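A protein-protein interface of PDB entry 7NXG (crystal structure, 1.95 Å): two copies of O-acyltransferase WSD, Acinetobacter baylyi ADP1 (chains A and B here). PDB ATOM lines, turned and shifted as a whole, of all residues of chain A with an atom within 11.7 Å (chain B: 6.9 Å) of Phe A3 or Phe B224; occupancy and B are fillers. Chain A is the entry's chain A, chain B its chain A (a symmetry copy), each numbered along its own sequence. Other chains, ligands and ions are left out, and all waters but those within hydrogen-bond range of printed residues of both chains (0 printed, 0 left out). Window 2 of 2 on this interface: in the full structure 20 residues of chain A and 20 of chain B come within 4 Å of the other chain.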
ATOM      1  N   ALA A   1      -1.478  -5.547  -5.104  1.00  0.00           N
ATOM      2  CA  ALA A   1      -1.850  -6.288  -3.880  1.00  0.00           C
ATOM      3  C   ALA A   1      -2.438  -7.636  -4.266  1.00  0.00           C
ATOM      4  O   ALA A   1      -2.567  -7.961  -5.452  1.00  0.00           O
ATOM      5  CB  ALA A   1      -2.848  -5.486  -3.042  1.00  0.00           C
ATOM      6  N   TYR A   2      -2.808  -8.410  -3.248  1.00  0.00           N
ATOM      7  CA  TYR A   2      -3.401  -9.731  -3.425  1.00  0.00           C
ATOM      8  C   TYR A   2      -4.880  -9.615  -3.084  1.00  0.00           C
ATOM      9  O   TYR A   2      -5.260  -9.572  -1.908  1.00  0.00           O
ATOM     10  CB  TYR A   2      -2.693 -10.769  -2.566  1.00  0.00           C
ATOM     11  CG  TYR A   2      -1.210 -10.859  -2.825  1.00  0.00           C
ATOM     12  CD1 TYR A   2      -0.721 -11.626  -3.876  1.00  0.00           C
ATOM     13  CD2 TYR A   2      -0.293 -10.179  -2.028  1.00  0.00           C
ATOM     14  CE1 TYR A   2       0.637 -11.718  -4.131  1.00  0.00           C
ATOM     15  CE2 TYR A   2       1.073 -10.258  -2.278  1.00  0.00           C
ATOM     16  CZ  TYR A   2       1.531 -11.034  -3.332  1.00  0.00           C
ATOM     17  OH  TYR A   2       2.875 -11.133  -3.599  1.00  0.00           O
ATOM     18  N   PHE A   3      -5.707  -9.527  -4.122  1.00  0.00           N
ATOM     19  CA  PHE A   3      -7.155  -9.489  -3.955  1.00  0.00           C
ATOM     20  C   PHE A   3      -7.570  -8.348  -3.034  1.00  0.00           C
ATOM     21  O   PHE A   3      -8.529  -8.465  -2.265  1.00  0.00           O
ATOM     22  CB  PHE A   3      -7.669 -10.835  -3.435  1.00  0.00           C
ATOM     23  CG  PHE A   3      -7.191 -12.014  -4.244  1.00  0.00           C
ATOM     24  CD1 PHE A   3      -7.920 -12.472  -5.336  1.00  0.00           C
ATOM     25  CD2 PHE A   3      -6.011 -12.667  -3.913  1.00  0.00           C
ATOM     26  CE1 PHE A   3      -7.482 -13.559  -6.079  1.00  0.00           C
ATOM     27  CE2 PHE A   3      -5.564 -13.751  -4.652  1.00  0.00           C
ATOM     28  CZ  PHE A   3      -6.297 -14.202  -5.734  1.00  0.00           C
ATOM     29  N   ALA A   4      -6.842  -7.236  -3.107  1.00  0.00           N
ATOM     30  CA  ALA A   4      -7.186  -6.027  -2.366  1.00  0.00           C
ATOM     31  C   ALA A   4      -7.348  -6.292  -0.875  1.00  0.00           C
ATOM     32  O   ALA A   4      -8.471  -6.350  -0.366  1.00  0.00           O
ATOM     33  CB  ALA A   4      -8.476  -5.419  -2.921  1.00  0.00           C
ATOM     34  N   GLY A   5      -6.234  -6.465  -0.172  1.00  0.00           N
ATOM     35  CA  GLY A   5      -6.218  -6.529   1.274  1.00  0.00           C
ATOM     36  C   GLY A   5      -5.877  -7.887   1.841  1.00  0.00           C
ATOM     37  O   GLY A   5      -5.575  -7.978   3.037  1.00  0.00           O
ATOM     38  N   MET A   6      -5.926  -8.944   1.031  1.00  0.00           N
ATOM     39  CA  MET A   6      -5.613 -10.258   1.545  1.00  0.00           C
ATOM     40  C   MET A   6      -4.102 -10.469   1.577  1.00  0.00           C
ATOM     41  O   MET A   6      -3.336  -9.756   0.925  1.00  0.00           O
ATOM     42  CB  MET A   6      -6.275 -11.333   0.683  1.00  0.00           C
ATOM     43  CG  MET A   6      -7.795 -11.313   0.739  1.00  0.00           C
ATOM     44  SD  MET A   6      -8.564 -12.699  -0.158  1.00  0.00           S
ATOM     45  CE  MET A   6     -10.149 -11.997  -0.574  1.00  0.00           C
ATOM     46  N   ARG A   7      -3.689 -11.500   2.311  1.00  0.00           N
ATOM     47  CA  ARG A   7      -2.288 -11.812   2.542  1.00  0.00           C
ATOM     48  C   ARG A   7      -2.053 -13.273   2.181  1.00  0.00           C
ATOM     49  O   ARG A   7      -2.836 -14.136   2.603  1.00  0.00           O
ATOM     50  CB  ARG A   7      -1.940 -11.562   4.042  1.00  0.00           C
ATOM     51  CG  ARG A   7      -0.514 -11.949   4.495  1.00  0.00           C
ATOM     52  CD  ARG A   7      -0.196 -11.539   5.955  1.00  0.00           C
ATOM     53  NE  ARG A   7      -0.267 -12.634   6.922  1.00  0.00           N
ATOM     54  CZ  ARG A   7      -1.257 -12.814   7.791  1.00  0.00           C
ATOM     55  NH1 ARG A   7      -2.293 -11.992   7.843  1.00  0.00           N
ATOM     56  NH2 ARG A   7      -1.204 -13.844   8.641  1.00  0.00           N
ATOM     57  N   PRO A   8      -1.035 -13.596   1.375  1.00  0.00           N
ATOM     58  CA  PRO A   8      -0.747 -15.007   1.090  1.00  0.00           C
ATOM     59  C   PRO A   8      -0.367 -15.738   2.362  1.00  0.00           C
ATOM     60  O   PRO A   8       0.295 -15.168   3.231  1.00  0.00           O
ATOM     61  CB  PRO A   8       0.440 -14.951   0.127  1.00  0.00           C
ATOM     62  CG  PRO A   8       0.458 -13.559  -0.387  1.00  0.00           C
ATOM     63  CD  PRO A   8      -0.080 -12.706   0.702  1.00  0.00           C
ATOM     64  N   LEU A   9      -0.766 -17.006   2.458  1.00  0.00           N
ATOM     65  CA  LEU A   9      -0.305 -17.854   3.555  1.00  0.00           C
ATOM     66  C   LEU A   9       1.218 -17.906   3.565  1.00  0.00           C
ATOM     67  O   LEU A   9       1.850 -17.921   2.508  1.00  0.00           O
ATOM     68  CB  LEU A   9      -0.829 -19.277   3.413  1.00  0.00           C
ATOM     69  CG  LEU A   9      -2.317 -19.523   3.520  1.00  0.00           C
ATOM     70  CD1 LEU A   9      -2.536 -21.033   3.501  1.00  0.00           C
ATOM     71  CD2 LEU A   9      -2.861 -18.891   4.767  1.00  0.00           C
ATOM     72  N   LYS A  66      -9.423 -15.268   8.386  1.00  0.00           N
ATOM     73  CA  LYS A  66      -9.989 -16.546   7.961  1.00  0.00           C
ATOM     74  C   LYS A  66      -9.400 -16.952   6.608  1.00  0.00           C
ATOM     75  O   LYS A  66      -8.974 -16.117   5.796  1.00  0.00           O
ATOM     76  CB  LYS A  66     -11.509 -16.492   7.886  1.00  0.00           C
ATOM     77  CG  LYS A  66     -11.972 -15.582   6.817  1.00  0.00           C
ATOM     78  CD  LYS A  66     -13.467 -15.515   6.744  1.00  0.00           C
ATOM     79  CE  LYS A  66     -14.058 -16.800   6.213  1.00  0.00           C
ATOM     80  NZ  LYS A  66     -15.506 -16.616   5.977  1.00  0.00           N
ATOM     81  N   LEU A  67      -9.459 -18.245   6.326  1.00  0.00           N
ATOM     82  CA  LEU A  67      -8.877 -18.750   5.092  1.00  0.00           C
ATOM     83  C   LEU A  67      -9.744 -18.408   3.878  1.00  0.00           C
ATOM     84  O   LEU A  67     -10.978 -18.420   3.940  1.00  0.00           O
ATOM     85  CB  LEU A  67      -8.707 -20.273   5.203  1.00  0.00           C
ATOM     86  CG  LEU A  67      -7.639 -20.757   6.200  1.00  0.00           C
ATOM     87  CD1 LEU A  67      -7.769 -22.248   6.458  1.00  0.00           C
ATOM     88  CD2 LEU A  67      -6.228 -20.411   5.710  1.00  0.00           C
ATOM     89  N   ASN A  68      -9.077 -18.102   2.760  1.00  0.00           N
ATOM     90  CA  ASN A  68      -9.741 -17.900   1.465  1.00  0.00           C
ATOM     91  C   ASN A  68      -8.751 -18.376   0.393  1.00  0.00           C
ATOM     92  O   ASN A  68      -7.886 -17.617  -0.062  1.00  0.00           O
ATOM     93  CB  ASN A  68     -10.139 -16.443   1.266  1.00  0.00           C
ATOM     94  CG  ASN A  68     -11.115 -16.227   0.101  1.00  0.00           C
ATOM     95  OD1 ASN A  68     -11.220 -17.035  -0.827  1.00  0.00           O
ATOM     96  ND2 ASN A  68     -11.832 -15.112   0.153  1.00  0.00           N
ATOM     97  N   GLY A  69      -8.870 -19.643   0.017  1.00  0.00           N
ATOM     98  CA  GLY A  69      -7.872 -20.233  -0.869  1.00  0.00           C
ATOM     99  C   GLY A  69      -6.537 -20.311  -0.153  1.00  0.00           C
ATOM    100  O   GLY A  69      -6.451 -20.762   0.986  1.00  0.00           O
ATOM    101  N   LEU A  70      -5.466 -19.922  -0.833  1.00  0.00           N
ATOM    102  CA  LEU A  70      -4.154 -19.875  -0.200  1.00  0.00           C
ATOM    103  C   LEU A  70      -3.850 -18.495   0.392  1.00  0.00           C
ATOM    104  O   LEU A  70      -2.702 -18.024   0.340  1.00  0.00           O
ATOM    105  CB  LEU A  70      -3.091 -20.297  -1.204  1.00  0.00           C
ATOM    106  CG  LEU A  70      -3.110 -21.785  -1.578  1.00  0.00           C
ATOM    107  CD1 LEU A  70      -2.080 -22.060  -2.660  1.00  0.00           C
ATOM    108  CD2 LEU A  70      -2.834 -22.686  -0.369  1.00  0.00           C
ATOM    109  N   PHE A  71      -4.861 -17.838   0.969  1.00  0.00           N
ATOM    110  CA  PHE A  71      -4.733 -16.470   1.446  1.00  0.00           C
ATOM    111  C   PHE A  71      -5.487 -16.300   2.752  1.00  0.00           C
ATOM    112  O   PHE A  71      -6.436 -17.033   3.036  1.00  0.00           O
ATOM    113  CB  PHE A  71      -5.287 -15.466   0.428  1.00  0.00           C
ATOM    114  CG  PHE A  71      -4.553 -15.475  -0.853  1.00  0.00           C
ATOM    115  CD1 PHE A  71      -4.838 -16.416  -1.827  1.00  0.00           C
ATOM    116  CD2 PHE A  71      -3.547 -14.561  -1.081  1.00  0.00           C
ATOM    117  CE1 PHE A  71      -4.142 -16.428  -3.023  1.00  0.00           C
ATOM    118  CE2 PHE A  71      -2.839 -14.564  -2.266  1.00  0.00           C
ATOM    119  CZ  PHE A  71      -3.133 -15.504  -3.240  1.00  0.00           C
ATOM    120  N   TRP A  72      -5.020 -15.344   3.557  1.00  0.00           N
ATOM    121  CA  TRP A  72      -5.731 -14.894   4.743  1.00  0.00           C
ATOM    122  C   TRP A  72      -6.606 -13.714   4.348  1.00  0.00           C
ATOM    123  O   TRP A  72      -6.117 -12.744   3.756  1.00  0.00           O
ATOM    124  CB  TRP A  72      -4.757 -14.487   5.850  1.00  0.00           C
ATOM    125  CG  TRP A  72      -3.993 -15.627   6.483  1.00  0.00           C
ATOM    126  CD1 TRP A  72      -2.653 -15.841   6.423  1.00  0.00           C
ATOM    127  CD2 TRP A  72      -4.532 -16.702   7.270  1.00  0.00           C
ATOM    128  NE1 TRP A  72      -2.314 -16.975   7.119  1.00  0.00           N
ATOM    129  CE2 TRP A  72      -3.451 -17.517   7.658  1.00  0.00           C
ATOM    130  CE3 TRP A  72      -5.816 -17.046   7.689  1.00  0.00           C
ATOM    131  CZ2 TRP A  72      -3.612 -18.651   8.431  1.00  0.00           C
ATOM    132  CZ3 TRP A  72      -5.977 -18.198   8.477  1.00  0.00           C
ATOM    133  CH2 TRP A  72      -4.876 -18.974   8.837  1.00  0.00           C
ATOM    134  N   ASP A  73      -7.894 -13.816   4.644  1.00  0.00           N
ATOM    135  CA  ASP A  73      -8.908 -12.801   4.376  1.00  0.00           C
ATOM    136  C   ASP A  73      -9.494 -12.356   5.716  1.00  0.00           C
ATOM    137  O   ASP A  73      -9.228 -12.964   6.752  1.00  0.00           O
ATOM    138  CB  ASP A  73      -9.992 -13.365   3.449  1.00  0.00           C
ATOM    139  CG  ASP A  73     -10.925 -12.288   2.866  1.00  0.00           C
ATOM    140  OD1 ASP A  73     -10.666 -11.075   2.992  1.00  0.00           O
ATOM    141  OD2 ASP A  73     -11.950 -12.687   2.277  1.00  0.00           O
ATOM    142  N   GLU A  74     -10.272 -11.279   5.700  1.00  0.00           N
ATOM    143  CA  GLU A  74     -10.889 -10.744   6.912  1.00  0.00           C
ATOM    144  C   GLU A  74     -12.301 -11.302   7.082  1.00  0.00           C
ATOM    145  O   GLU A  74     -13.098 -11.319   6.128  1.00  0.00           O
ATOM    146  CB  GLU A  74     -10.913  -9.218   6.892  1.00  0.00           C
ATOM    147  CG  GLU A  74      -9.532  -8.623   7.104  1.00  0.00           C
ATOM    148  CD  GLU A  74      -9.577  -7.199   7.580  1.00  0.00           C
ATOM    149  OE1 GLU A  74     -10.410  -6.422   7.066  1.00  0.00           O
ATOM    150  OE2 GLU A  74      -8.768  -6.856   8.465  1.00  0.00           O
ATOM    151  N   SER B 223     -12.242  -6.550  -7.871  1.00  0.00           N
ATOM    152  CA  SER B 223     -11.124  -7.460  -7.630  1.00  0.00           C
ATOM    153  C   SER B 223     -11.362  -8.842  -8.251  1.00  0.00           C
ATOM    154  O   SER B 223     -10.417  -9.609  -8.462  1.00  0.00           O
ATOM    155  CB  SER B 223     -10.871  -7.587  -6.134  1.00  0.00           C
ATOM    156  N   PHE B 224     -12.636  -9.164  -8.506  1.00  0.00           N
ATOM    157  CA  PHE B 224     -13.063 -10.407  -9.168  1.00  0.00           C
ATOM    158  C   PHE B 224     -13.973 -10.004 -10.334  1.00  0.00           C
ATOM    159  O   PHE B 224     -15.197  -9.983 -10.193  1.00  0.00           O
ATOM    160  CB  PHE B 224     -13.773 -11.364  -8.203  1.00  0.00           C
ATOM    161  CG  PHE B 224     -12.952 -11.771  -7.017  1.00  0.00           C
ATOM    162  CD1 PHE B 224     -12.079 -12.850  -7.094  1.00  0.00           C
ATOM    163  CD2 PHE B 224     -13.063 -11.092  -5.819  1.00  0.00           C
ATOM    164  CE1 PHE B 224     -11.325 -13.236  -5.996  1.00  0.00           C
ATOM    165  CE2 PHE B 224     -12.316 -11.468  -4.721  1.00  0.00           C
ATOM    166  CZ  PHE B 224     -11.443 -12.545  -4.812  1.00  0.00           C
ATOM    167  N   GLN B 225     -13.376  -9.674 -11.474  1.00  0.00           N
ATOM    168  CA  GLN B 225     -14.119  -9.178 -12.625  1.00  0.00           C
ATOM    169  C   GLN B 225     -14.343 -10.221 -13.710  1.00  0.00           C
ATOM    170  O   GLN B 225     -14.942  -9.895 -14.741  1.00  0.00           O
ATOM    171  CB  GLN B 225     -13.394  -7.980 -13.236  1.00  0.00           C
ATOM    172  CG  GLN B 225     -13.238  -6.805 -12.291  1.00  0.00           C
ATOM    173  CD  GLN B 225     -12.209  -5.807 -12.783  1.00  0.00           C
ATOM    174  OE1 GLN B 225     -11.546  -6.029 -13.797  1.00  0.00           O
ATOM    175  NE2 GLN B 225     -12.064  -4.706 -12.062  1.00  0.00           N
ATOM    176  N   ALA B 226     -13.920 -11.461 -13.497  1.00  0.00           N
ATOM    177  CA  ALA B 226     -14.005 -12.489 -14.528  1.00  0.00           C
ATOM    178  C   ALA B 226     -15.392 -13.130 -14.535  1.00  0.00           C
ATOM    179  O   ALA B 226     -15.895 -13.519 -13.476  1.00  0.00           O
ATOM    180  CB  ALA B 226     -12.933 -13.560 -14.314  1.00  0.00           C
ATOM    181  N   PRO B 227     -16.036 -13.249 -15.692  1.00  0.00           N
ATOM    182  CA  PRO B 227     -17.370 -13.859 -15.741  1.00  0.00           C
ATOM    183  C   PRO B 227     -17.307 -15.372 -15.558  1.00  0.00           C
ATOM    184  O   PRO B 227     -16.248 -15.982 -15.674  1.00  0.00           O
ATOM    185  CB  PRO B 227     -17.851 -13.507 -17.155  1.00  0.00           C
ATOM    186  CG  PRO B 227     -16.593 -13.469 -17.977  1.00  0.00           C
ATOM    187  CD  PRO B 227     -15.537 -12.902 -17.041  1.00  0.00           C
ATOM    188  N   LYS B 287     -19.622 -10.497 -20.464  1.00  0.00           N
ATOM    189  CA  LYS B 287     -18.424  -9.756 -20.073  1.00  0.00           C
ATOM    190  C   LYS B 287     -17.186 -10.352 -20.758  1.00  0.00           C
ATOM    191  O   LYS B 287     -17.159 -11.544 -21.067  1.00  0.00           O
ATOM    192  CB  LYS B 287     -18.219  -9.832 -18.567  1.00  0.00           C
ATOM    193  CG  LYS B 287     -19.260  -9.118 -17.726  1.00  0.00           C
ATOM    194  CD  LYS B 287     -18.933  -9.191 -16.234  1.00  0.00           C
ATOM    195  CE  LYS B 287     -17.688  -8.377 -15.882  1.00  0.00           C
ATOM    196  NZ  LYS B 287     -17.553  -8.132 -14.417  1.00  0.00           N
ATOM    197  N   ILE B 290     -11.091 -12.426 -18.664  1.00  0.00           N
ATOM    198  CA  ILE B 290      -9.886 -11.901 -18.025  1.00  0.00           C
ATOM    199  C   ILE B 290      -8.858 -13.017 -18.015  1.00  0.00           C
ATOM    200  O   ILE B 290      -9.220 -14.180 -17.762  1.00  0.00           O
ATOM    201  CB  ILE B 290     -10.168 -11.424 -16.589  1.00  0.00           C
ATOM    202  CG1 ILE B 290     -11.319 -10.429 -16.576  1.00  0.00           C
ATOM    203  CG2 ILE B 290      -8.898 -10.860 -15.976  1.00  0.00           C
ATOM    204  CD1 ILE B 290     -11.081  -9.235 -17.421  1.00  0.00           C
ATOM    205  N   GLN B 338      -2.296  -5.164 -11.549  1.00  0.00           N
ATOM    206  CA  GLN B 338      -2.046  -6.503 -11.003  1.00  0.00           C
ATOM    207  C   GLN B 338      -0.901  -7.133 -11.780  1.00  0.00           C
ATOM    208  O   GLN B 338      -1.112  -7.828 -12.775  1.00  0.00           O
ATOM    209  CB  GLN B 338      -3.296  -7.377 -11.060  1.00  0.00           C
ATOM    210  CG  GLN B 338      -4.332  -7.051 -10.017  1.00  0.00           C
ATOM    211  CD  GLN B 338      -5.163  -5.864 -10.402  1.00  0.00           C
ATOM    212  OE1 GLN B 338      -6.169  -5.989 -11.104  1.00  0.00           O
ATOM    213  NE2 GLN B 338      -4.750  -4.689  -9.935  1.00  0.00           N
ATOM    214  N   PHE B 340       2.740  -9.371 -11.448  1.00  0.00           N
ATOM    215  CA  PHE B 340       3.350 -10.391 -10.587  1.00  0.00           C
ATOM    216  C   PHE B 340       4.737 -10.743 -11.113  1.00  0.00           C
ATOM    217  O   PHE B 340       4.885 -11.547 -12.039  1.00  0.00           O
ATOM    218  CB  PHE B 340       2.466 -11.627 -10.521  1.00  0.00           C
ATOM    219  CG  PHE B 340       1.083 -11.335 -10.052  1.00  0.00           C
ATOM    220  CD1 PHE B 340       0.781 -11.340  -8.704  1.00  0.00           C
ATOM    221  CD2 PHE B 340       0.085 -11.030 -10.962  1.00  0.00           C
ATOM    222  CE1 PHE B 340      -0.497 -11.056  -8.264  1.00  0.00           C
ATOM    223  CE2 PHE B 340      -1.192 -10.744 -10.529  1.00  0.00           C
ATOM    224  CZ  PHE B 340      -1.484 -10.760  -9.179  1.00  0.00           C
ATOM    225  N   ALA B 353       0.600 -19.085  -5.643  1.00  0.00           N
ATOM    226  CA  ALA B 353      -0.610 -19.090  -4.819  1.00  0.00           C
ATOM    227  C   ALA B 353      -1.776 -18.439  -5.558  1.00  0.00           C
ATOM    228  O   ALA B 353      -2.911 -18.939  -5.520  1.00  0.00           O
ATOM    229  CB  ALA B 353      -0.348 -18.382  -3.495  1.00  0.00           C
ATOM    230  N   VAL B 354      -1.523 -17.290  -6.196  1.00  0.00           N
ATOM    231  CA  VAL B 354      -2.561 -16.636  -6.993  1.00  0.00           C
ATOM    232  C   VAL B 354      -3.131 -17.594  -8.025  1.00  0.00           C
ATOM    233  O   VAL B 354      -4.352 -17.740  -8.151  1.00  0.00           O
ATOM    234  CB  VAL B 354      -1.993 -15.385  -7.680  1.00  0.00           C
ATOM    235  CG1 VAL B 354      -2.988 -14.849  -8.711  1.00  0.00           C
ATOM    236  CG2 VAL B 354      -1.638 -14.349  -6.633  1.00  0.00           C
ATOM    237  N   VAL B 355      -2.251 -18.288  -8.755  1.00  0.00           N
ATOM    238  CA  VAL B 355      -2.678 -19.042  -9.929  1.00  0.00           C
ATOM    239  C   VAL B 355      -3.273 -20.390  -9.552  1.00  0.00           C
ATOM    240  O   VAL B 355      -4.272 -20.826 -10.139  1.00  0.00           O
ATOM    241  CB  VAL B 355      -1.485 -19.214 -10.893  1.00  0.00           C
ATOM    242  CG1 VAL B 355      -1.748 -20.341 -11.886  1.00  0.00           C
ATOM    243  CG2 VAL B 355      -1.217 -17.902 -11.623  1.00  0.00           C
ATOM    244  N   GLY B 357      -4.025 -21.519  -6.255  1.00  0.00           N
ATOM    245  CA  GLY B 357      -4.910 -21.492  -5.105  1.00  0.00           C
ATOM    246  C   GLY B 357      -5.585 -20.144  -4.927  1.00  0.00           C
ATOM    247  O   GLY B 357      -5.599 -19.567  -3.835  1.00  0.00           O
ATOM    248  N   PRO B 358      -6.226 -19.643  -5.988  1.00  0.00           N
ATOM    249  CA  PRO B 358      -6.801 -18.295  -5.923  1.00  0.00           C
ATOM    250  C   PRO B 358      -7.919 -18.175  -4.895  1.00  0.00           C
ATOM    251  O   PRO B 358      -8.695 -19.104  -4.671  1.00  0.00           O
ATOM    252  CB  PRO B 358      -7.321 -18.069  -7.349  1.00  0.00           C
ATOM    253  CG  PRO B 358      -7.603 -19.444  -7.862  1.00  0.00           C
ATOM    254  CD  PRO B 358      -6.546 -20.324  -7.257  1.00  0.00           C
ATOM    255  N   ALA B 359      -7.963 -17.028  -4.224  1.00  0.00           N
ATOM    256  CA  ALA B 359      -9.119 -16.697  -3.409  1.00  0.00           C
ATOM    257  C   ALA B 359     -10.341 -16.478  -4.300  1.00  0.00           C
ATOM    258  O   ALA B 359     -10.223 -16.192  -5.495  1.00  0.00           O
ATOM    259  CB  ALA B 359      -8.846 -15.457  -2.560  1.00  0.00           C
ATOM    260  N   GLY B 360     -11.531 -16.600  -3.695  1.00  0.00           N
ATOM    261  CA  GLY B 360     -12.777 -16.456  -4.417  1.00  0.00           C
ATOM    262  C   GLY B 360     -13.714 -15.465  -3.745  1.00  0.00           C
ATOM    263  O   GLY B 360     -13.466 -14.990  -2.632  1.00  0.00           O
ATOM    264  N   LEU B 361     -14.803 -15.159  -4.446  1.00  0.00           N
ATOM    265  CA  LEU B 361     -15.788 -14.196  -3.948  1.00  0.00           C
ATOM    266  C   LEU B 361     -16.645 -14.819  -2.857  1.00  0.00           C
ATOM    267  O   LEU B 361     -17.485 -15.678  -3.130  1.00  0.00           O
ATOM    268  CB  LEU B 361     -16.673 -13.696  -5.074  1.00  0.00           C
ATOM    269  N   GLN B 372     -14.649 -15.606 -10.066  1.00  0.00           N
ATOM    270  CA  GLN B 372     -13.215 -15.836  -9.953  1.00  0.00           C
ATOM    271  C   GLN B 372     -12.439 -14.594 -10.414  1.00  0.00           C
ATOM    272  O   GLN B 372     -13.018 -13.626 -10.917  1.00  0.00           O
ATOM    273  CB  GLN B 372     -12.801 -17.077 -10.774  1.00  0.00           C
ATOM    274  N   ALA B 373     -11.118 -14.631 -10.223  1.00  0.00           N
ATOM    275  CA  ALA B 373     -10.264 -13.497 -10.554  1.00  0.00           C
ATOM    276  C   ALA B 373      -9.912 -13.448 -12.045  1.00  0.00           C
ATOM    277  O   ALA B 373      -9.806 -12.360 -12.629  1.00  0.00           O
ATOM    278  CB  ALA B 373      -8.991 -13.555  -9.710  1.00  0.00           C
ATOM    279  N   PHE B 374      -9.715 -14.610 -12.669  1.00  0.00           N
ATOM    280  CA  PHE B 374      -9.353 -14.702 -14.077  1.00  0.00           C
ATOM    281  C   PHE B 374      -9.979 -15.963 -14.656  1.00  0.00           C
ATOM    282  O   PHE B 374     -10.384 -16.873 -13.918  1.00  0.00           O
ATOM    283  CB  PHE B 374      -7.831 -14.724 -14.259  1.00  0.00           C
ATOM    284  CG  PHE B 374      -7.128 -15.764 -13.412  1.00  0.00           C
ATOM    285  CD1 PHE B 374      -6.754 -15.477 -12.116  1.00  0.00           C
ATOM    286  CD2 PHE B 374      -6.865 -17.023 -13.906  1.00  0.00           C
ATOM    287  CE1 PHE B 374      -6.112 -16.439 -11.332  1.00  0.00           C
ATOM    288  CE2 PHE B 374      -6.221 -17.987 -13.129  1.00  0.00           C
ATOM    289  CZ  PHE B 374      -5.846 -17.698 -11.856  1.00  0.00           C
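OD1 of Asn A68 sits at hydrogen-bond distance from N of Gly B360, 2.9 Å away. N of Leu A70 lies within hydrogen-bond range of O of Gly B357 (3.0 Å).
O of Leu A70 lies within hydrogen-bond range of N of Leu A9, at 3.0 Å. ND2 of Asn A68 lies within hydrogen-bond range of OD2 of Asp A73, at 3.2 Å.
CG2 of Val B354 touches CD1 of Tyr A2, at 3.98 Å. CD1 of Phe A3 touches CE1 of Phe B224, at 3.6 Å. N of Ala B359 touches CZ of Phe A3, at 3.6 Å. Phe A3 touches Ala B373 (CE1 to CB, 3.9 Å). Ala B359 touches Met A6 (CB to SD, 3.7 Å). OD1 of Asn A68 touches CB of Ala B359 (3.3 Å). Gly A69 touches Gly B357. CA of Ala B353 touches CD1 of Leu A70 (3.96 Å). Gly B357 touches Phe A71. Phe A71 touches Ala B359 (CD1 to N, 3.99 Å).
Of the printed residues of chain B, Phe A3 touches Phe B224, Ala B359 and Ala B373. Phe B224 touches one residue of chain A. No residue of chain A comes within 4 Å of Ser B223. No residue of chain A comes within 4 Å of Gln B225. No residue of chain A comes within 4 Å of Ala B226. No residue of chain A comes within 4 Å of Pro B358. Of chain A, only Phe A3 (3.9 Å) comes within 4 Å of Ala B373. Of the printed residues of chain B, Gly A69 touches Gly B357. Of the printed residues of chain B, Phe A71 touches Ala B353 (3.7 Å), Val B354 (3.8 Å), Gly B357 (3.6 Å) and Ala B359 (3.99 Å). Printed residues of chain A within 4 Å of Gly B357: Gly A69, Leu A70 and Phe A71. Ala A4 touches none of the printed residues of chain B. Leu A67 touches none of the printed residues of chain B. The nearest residue of chain A that does not touch Phe B224 is Met A6 (4.5 Å).
Hydrophobic or aromatic side chains of chain B within 4 Å of the printed part of chain A: Phe B224, Val B354, Ala B359 and Ala B373. Hydrophobic or aromatic side chains of chain A that line the printed part of chain B: Tyr A2, Phe A3, Met A6, Leu A70 and Phe A71. Among the printed residues, 14 pairs touch across the chains. Among the printed residues, no Asp or Glu carboxylate lies within 4 Å of a Lys or Arg side-chain nitrogen of the other chain.
No position is printed for both chains. Of the 14 pairs that touch across the chains among the printed residues, none has its exchanged pair printed and touching as well.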
